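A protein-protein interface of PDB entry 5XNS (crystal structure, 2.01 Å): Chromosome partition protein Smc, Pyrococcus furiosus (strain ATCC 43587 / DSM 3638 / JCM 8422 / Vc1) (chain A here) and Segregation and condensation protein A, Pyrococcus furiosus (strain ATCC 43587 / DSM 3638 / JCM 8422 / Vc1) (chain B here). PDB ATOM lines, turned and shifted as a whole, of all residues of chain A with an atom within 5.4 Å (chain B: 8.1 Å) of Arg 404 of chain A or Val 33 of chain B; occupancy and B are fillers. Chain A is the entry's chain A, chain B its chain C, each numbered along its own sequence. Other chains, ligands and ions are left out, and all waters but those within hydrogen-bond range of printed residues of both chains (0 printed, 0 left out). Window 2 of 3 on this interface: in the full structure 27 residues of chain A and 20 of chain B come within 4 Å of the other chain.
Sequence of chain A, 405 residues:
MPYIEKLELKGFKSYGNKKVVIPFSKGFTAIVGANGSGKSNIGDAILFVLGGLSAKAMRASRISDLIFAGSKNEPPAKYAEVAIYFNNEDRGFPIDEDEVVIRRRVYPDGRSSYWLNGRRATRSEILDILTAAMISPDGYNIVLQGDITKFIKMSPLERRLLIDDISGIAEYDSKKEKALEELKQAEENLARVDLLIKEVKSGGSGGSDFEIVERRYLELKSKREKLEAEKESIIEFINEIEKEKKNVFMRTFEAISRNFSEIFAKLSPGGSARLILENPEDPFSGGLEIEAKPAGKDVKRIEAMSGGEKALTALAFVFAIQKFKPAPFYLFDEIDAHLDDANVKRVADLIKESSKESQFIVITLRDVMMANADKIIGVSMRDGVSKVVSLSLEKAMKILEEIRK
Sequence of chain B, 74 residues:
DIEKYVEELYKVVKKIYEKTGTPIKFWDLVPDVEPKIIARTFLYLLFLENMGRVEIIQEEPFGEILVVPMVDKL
Among the printed residues, merely in contact across the chains: Met 397 of chain A with Val 33 of chain B, Met 397 of chain A with Pro 35 of chain B, Met 397 of chain A with Ile 38 of chain B, Leu 400 of chain A with Val 30 of chain B, Leu 400 of chain A with Val 33 of chain B, Leu 400 of chain A with Ile 38 of chain B, Glu 401 of chain A with Val 33 of chain B and Arg 404 of chain A with Val 33 of chain B.
Of the 8 printed residues of chain A, 4 touch a printed residue of chain B.
Hydrophobic or aromatic side chains of chain A that line the printed part of chain B: Met 397 and Leu 400.
Printed residues of chain B that touch a printed residue of chain A: Val 30, Val 33, Pro 35 and Ile 38.
Hydrophobic or aromatic side chains of chain B that line the printed part of chain A: Val 30, Val 33, Pro 35 and Ile 38.
Among the printed residues, no Asp or Glu carboxylate lies within 4 Å of a Lys or Arg side-chain nitrogen of the other chain.
Printed residues of chain B within 4 Å of Met 397 of chain A: Val 33, Pro 35 and Ile 38.
Of the printed residues of chain B, Glu 401 of chain A touches Val 33 (3.5 Å).
Arg 404 of chain A touches just one residue of chain B: Val 33 (3.7 Å).
Of the printed residues of chain A, Val 33 of chain B touches Met 397, Leu 400, Glu 401 and Arg 404.
Of the printed residues of chain A, Pro 35 of chain B touches Met 397 (3.7 Å).
Of the printed residues of chain A, Ile 38 of chain B touches Met 397 and Leu 400.
The nearest residue of chain B that does not touch Arg 404 of chain A is Pro 31 of chain B (4.2 Å).
The nearest printed residue of chain A that does not touch Val 30 of chain B is Arg 404 of chain A (6.2 Å).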
ATOM      1  N   MET A 397     -26.952 -13.230  -3.881  1.00  0.00           N
ATOM      2  CA  MET A 397     -27.415 -13.222  -2.498  1.00  0.00           C
ATOM      3  C   MET A 397     -26.249 -13.057  -1.534  1.00  0.00           C
ATOM      4  O   MET A 397     -26.301 -12.238  -0.613  1.00  0.00           O
ATOM      5  CB  MET A 397     -28.191 -14.504  -2.190  1.00  0.00           C
ATOM      6  CG  MET A 397     -29.617 -14.493  -2.719  1.00  0.00           C
ATOM      7  SD  MET A 397     -30.570 -13.127  -2.021  1.00  0.00           S
ATOM      8  CE  MET A 397     -31.179 -13.884  -0.512  1.00  0.00           C
ATOM      9  N   ILE A 399     -23.135 -11.808  -2.151  1.00  0.00           N
ATOM     10  CA  ILE A 399     -22.466 -10.512  -2.302  1.00  0.00           C
ATOM     11  C   ILE A 399     -23.259  -9.404  -1.616  1.00  0.00           C
ATOM     12  O   ILE A 399     -22.680  -8.520  -0.971  1.00  0.00           O
ATOM     13  CB  ILE A 399     -22.220 -10.197  -3.791  1.00  0.00           C
ATOM     14  CG1 ILE A 399     -21.087 -11.072  -4.339  1.00  0.00           C
ATOM     15  CG2 ILE A 399     -21.899  -8.712  -3.981  1.00  0.00           C
ATOM     16  CD1 ILE A 399     -20.750 -10.834  -5.786  1.00  0.00           C
ATOM     17  N   LEU A 400     -24.589  -9.451  -1.711  1.00  0.00           N
ATOM     18  CA  LEU A 400     -25.416  -8.386  -1.152  1.00  0.00           C
ATOM     19  C   LEU A 400     -25.610  -8.536   0.355  1.00  0.00           C
ATOM     20  O   LEU A 400     -25.640  -7.531   1.075  1.00  0.00           O
ATOM     21  CB  LEU A 400     -26.766  -8.345  -1.864  1.00  0.00           C
ATOM     22  CG  LEU A 400     -26.662  -7.846  -3.303  1.00  0.00           C
ATOM     23  CD1 LEU A 400     -27.941  -8.162  -4.058  1.00  0.00           C
ATOM     24  CD2 LEU A 400     -26.381  -6.351  -3.309  1.00  0.00           C
ATOM     25  N   GLU A 401     -25.775  -9.768   0.846  1.00  0.00           N
ATOM     26  CA  GLU A 401     -25.792  -9.997   2.291  1.00  0.00           C
ATOM     27  C   GLU A 401     -24.536  -9.426   2.942  1.00  0.00           C
ATOM     28  O   GLU A 401     -24.607  -8.770   3.990  1.00  0.00           O
ATOM     29  CB  GLU A 401     -25.916 -11.496   2.587  1.00  0.00           C
ATOM     30  CG  GLU A 401     -27.311 -12.067   2.335  1.00  0.00           C
ATOM     31  CD  GLU A 401     -27.352 -13.600   2.220  1.00  0.00           C
ATOM     32  OE1 GLU A 401     -26.354 -14.218   1.770  1.00  0.00           O
ATOM     33  OE2 GLU A 401     -28.404 -14.186   2.561  1.00  0.00           O
ATOM     34  N   GLU A 402     -23.378  -9.646   2.314  1.00  0.00           N
ATOM     35  CA  GLU A 402     -22.125  -9.108   2.830  1.00  0.00           C
ATOM     36  C   GLU A 402     -22.068  -7.584   2.715  1.00  0.00           C
ATOM     37  O   GLU A 402     -21.470  -6.923   3.571  1.00  0.00           O
ATOM     38  CB  GLU A 402     -20.953  -9.775   2.108  1.00  0.00           C
ATOM     39  CG  GLU A 402     -19.609  -9.098   2.290  1.00  0.00           C
ATOM     40  CD  GLU A 402     -19.087  -9.154   3.728  1.00  0.00           C
ATOM     41  OE1 GLU A 402     -18.214  -8.318   4.065  1.00  0.00           O
ATOM     42  OE2 GLU A 402     -19.540 -10.020   4.516  1.00  0.00           O
ATOM     43  N   ILE A 403     -22.693  -7.001   1.687  1.00  0.00           N
ATOM     44  CA  ILE A 403     -22.743  -5.541   1.598  1.00  0.00           C
ATOM     45  C   ILE A 403     -23.658  -4.972   2.680  1.00  0.00           C
ATOM     46  O   ILE A 403     -23.472  -3.833   3.128  1.00  0.00           O
ATOM     47  CB  ILE A 403     -23.173  -5.104   0.178  1.00  0.00           C
ATOM     48  CG1 ILE A 403     -22.078  -5.424  -0.844  1.00  0.00           C
ATOM     49  CG2 ILE A 403     -23.485  -3.622   0.110  1.00  0.00           C
ATOM     50  CD1 ILE A 403     -22.459  -5.060  -2.262  1.00  0.00           C
ATOM     51  N   ARG A 404     -24.623  -5.764   3.158  1.00  0.00           N
ATOM     52  CA  ARG A 404     -25.521  -5.362   4.242  1.00  0.00           C
ATOM     53  C   ARG A 404     -24.750  -5.227   5.563  1.00  0.00           C
ATOM     54  O   ARG A 404     -25.302  -5.413   6.652  1.00  0.00           O
ATOM     55  CB  ARG A 404     -26.684  -6.373   4.336  1.00  0.00           C
ATOM     56  CG  ARG A 404     -27.788  -6.081   5.364  1.00  0.00           C
ATOM     57  CD  ARG A 404     -29.180  -6.241   4.792  1.00  0.00           C
ATOM     58  NE  ARG A 404     -29.518  -5.111   3.933  1.00  0.00           N
ATOM     59  CZ  ARG A 404     -30.673  -4.971   3.280  1.00  0.00           C
ATOM     60  NH1 ARG A 404     -31.625  -5.899   3.379  1.00  0.00           N
ATOM     61  NH2 ARG A 404     -30.881  -3.900   2.523  1.00  0.00           N
ATOM     62  N   LYS A 405     -23.463  -4.890   5.475  1.00  0.00           N
ATOM     63  CA  LYS A 405     -22.619  -4.654   6.637  1.00  0.00           C
ATOM     64  C   LYS A 405     -21.794  -3.388   6.397  1.00  0.00           C
ATOM     65  O   LYS A 405     -22.160  -2.285   6.822  1.00  0.00           O
ATOM     66  CB  LYS A 405     -21.704  -5.851   6.889  1.00  0.00           C
ATOM     67  CG  LYS A 405     -22.383  -7.211   6.720  1.00  0.00           C
ATOM     68  CD  LYS A 405     -23.419  -7.472   7.807  1.00  0.00           C
ATOM     69  CE  LYS A 405     -24.165  -8.771   7.556  1.00  0.00           C
ATOM     70  NZ  LYS A 405     -23.276  -9.950   7.746  1.00  0.00           N
ATOM     71  OXT LYS A 405     -20.746  -3.445   5.742  1.00  0.00           O
ATOM     72  N   VAL B  30     -29.408  -2.635  -6.436  1.00  0.00           N
ATOM     73  CA  VAL B  30     -30.420  -3.574  -5.959  1.00  0.00           C
ATOM     74  C   VAL B  30     -30.901  -3.155  -4.573  1.00  0.00           C
ATOM     75  O   VAL B  30     -30.107  -3.141  -3.620  1.00  0.00           O
ATOM     76  CB  VAL B  30     -29.868  -5.007  -5.939  1.00  0.00           C
ATOM     77  CG1 VAL B  30     -30.907  -5.965  -5.360  1.00  0.00           C
ATOM     78  CG2 VAL B  30     -29.429  -5.433  -7.344  1.00  0.00           C
ATOM     79  N   PRO B  31     -32.183  -2.818  -4.401  1.00  0.00           N
ATOM     80  CA  PRO B  31     -32.612  -2.197  -3.137  1.00  0.00           C
ATOM     81  C   PRO B  31     -32.893  -3.168  -1.995  1.00  0.00           C
ATOM     82  O   PRO B  31     -33.005  -2.708  -0.851  1.00  0.00           O
ATOM     83  CB  PRO B  31     -33.884  -1.427  -3.543  1.00  0.00           C
ATOM     84  CG  PRO B  31     -34.434  -2.189  -4.702  1.00  0.00           C
ATOM     85  CD  PRO B  31     -33.230  -2.756  -5.444  1.00  0.00           C
ATOM     86  N   ASP B  32     -32.992  -4.480  -2.236  1.00  0.00           N
ATOM     87  CA  ASP B  32     -33.222  -5.430  -1.147  1.00  0.00           C
ATOM     88  C   ASP B  32     -32.469  -6.720  -1.422  1.00  0.00           C
ATOM     89  O   ASP B  32     -32.298  -7.122  -2.577  1.00  0.00           O
ATOM     90  CB  ASP B  32     -34.713  -5.739  -0.952  1.00  0.00           C
ATOM     91  CG  ASP B  32     -35.524  -4.494  -0.628  1.00  0.00           C
ATOM     92  OD1 ASP B  32     -35.349  -3.950   0.488  1.00  0.00           O
ATOM     93  OD2 ASP B  32     -36.317  -4.048  -1.493  1.00  0.00           O
ATOM     94  N   VAL B  33     -32.039  -7.377  -0.346  1.00  0.00           N
ATOM     95  CA  VAL B  33     -31.340  -8.653  -0.446  1.00  0.00           C
ATOM     96  C   VAL B  33     -32.384  -9.760  -0.464  1.00  0.00           C
ATOM     97  O   VAL B  33     -32.529 -10.512   0.508  1.00  0.00           O
ATOM     98  CB  VAL B  33     -30.341  -8.846   0.711  1.00  0.00           C
ATOM     99  CG1 VAL B  33     -29.439 -10.045   0.444  1.00  0.00           C
ATOM    100  CG2 VAL B  33     -29.513  -7.593   0.913  1.00  0.00           C
ATOM    101  N   GLU B  34     -33.133  -9.852  -1.565  1.00  0.00           N
ATOM    102  CA  GLU B  34     -34.189 -10.838  -1.755  1.00  0.00           C
ATOM    103  C   GLU B  34     -34.115 -11.243  -3.222  1.00  0.00           C
ATOM    104  O   GLU B  34     -33.939 -10.366  -4.088  1.00  0.00           O
ATOM    105  CB  GLU B  34     -35.573 -10.280  -1.419  1.00  0.00           C
ATOM    106  CG  GLU B  34     -36.383 -11.160  -0.476  1.00  0.00           C
ATOM    107  CD  GLU B  34     -35.586 -11.597   0.761  1.00  0.00           C
ATOM    108  OE1 GLU B  34     -35.309 -12.823   0.877  1.00  0.00           O
ATOM    109  OE2 GLU B  34     -35.245 -10.711   1.593  1.00  0.00           O
ATOM    110  N   PRO B  35     -34.214 -12.543  -3.535  1.00  0.00           N
ATOM    111  CA  PRO B  35     -33.991 -12.969  -4.931  1.00  0.00           C
ATOM    112  C   PRO B  35     -34.932 -12.314  -5.924  1.00  0.00           C
ATOM    113  O   PRO B  35     -34.492 -11.979  -7.031  1.00  0.00           O
ATOM    114  CB  PRO B  35     -34.169 -14.502  -4.876  1.00  0.00           C
ATOM    115  CG  PRO B  35     -34.616 -14.823  -3.482  1.00  0.00           C
ATOM    116  CD  PRO B  35     -34.218 -13.685  -2.605  1.00  0.00           C
ATOM    117  N   LYS B  36     -36.202 -12.084  -5.550  1.00  0.00           N
ATOM    118  CA  LYS B  36     -37.137 -11.466  -6.476  1.00  0.00           C
ATOM    119  C   LYS B  36     -36.747 -10.029  -6.787  1.00  0.00           C
ATOM    120  O   LYS B  36     -37.014  -9.535  -7.886  1.00  0.00           O
ATOM    121  CB  LYS B  36     -38.553 -11.512  -5.920  1.00  0.00           C
ATOM    122  CG  LYS B  36     -39.615 -11.084  -6.924  1.00  0.00           C
ATOM    123  CD  LYS B  36     -41.046 -11.291  -6.408  1.00  0.00           C
ATOM    124  CE  LYS B  36     -41.332 -10.418  -5.192  1.00  0.00           C
ATOM    125  NZ  LYS B  36     -42.757 -10.491  -4.764  1.00  0.00           N
ATOM    126  N   ILE B  37     -36.131  -9.340  -5.833  1.00  0.00           N
ATOM    127  CA  ILE B  37     -35.769  -7.951  -6.061  1.00  0.00           C
ATOM    128  C   ILE B  37     -34.487  -7.866  -6.875  1.00  0.00           C
ATOM    129  O   ILE B  37     -34.359  -7.005  -7.752  1.00  0.00           O
ATOM    130  CB  ILE B  37     -35.659  -7.210  -4.717  1.00  0.00           C
ATOM    131  CG1 ILE B  37     -36.988  -7.301  -3.959  1.00  0.00           C
ATOM    132  CG2 ILE B  37     -35.290  -5.754  -4.938  1.00  0.00           C
ATOM    133  CD1 ILE B  37     -38.171  -6.761  -4.751  1.00  0.00           C
ATOM    134  N   ILE B  38     -33.527  -8.760  -6.611  1.00  0.00           N
ATOM    135  CA  ILE B  38     -32.375  -8.876  -7.500  1.00  0.00           C
ATOM    136  C   ILE B  38     -32.851  -9.133  -8.918  1.00  0.00           C
ATOM    137  O   ILE B  38     -32.452  -8.444  -9.861  1.00  0.00           O
ATOM    138  CB  ILE B  38     -31.417  -9.980  -7.023  1.00  0.00           C
ATOM    139  CG1 ILE B  38     -30.896  -9.672  -5.619  1.00  0.00           C
ATOM    140  CG2 ILE B  38     -30.242 -10.094  -7.980  1.00  0.00           C
ATOM    141  CD1 ILE B  38     -30.290 -10.865  -4.935  1.00  0.00           C
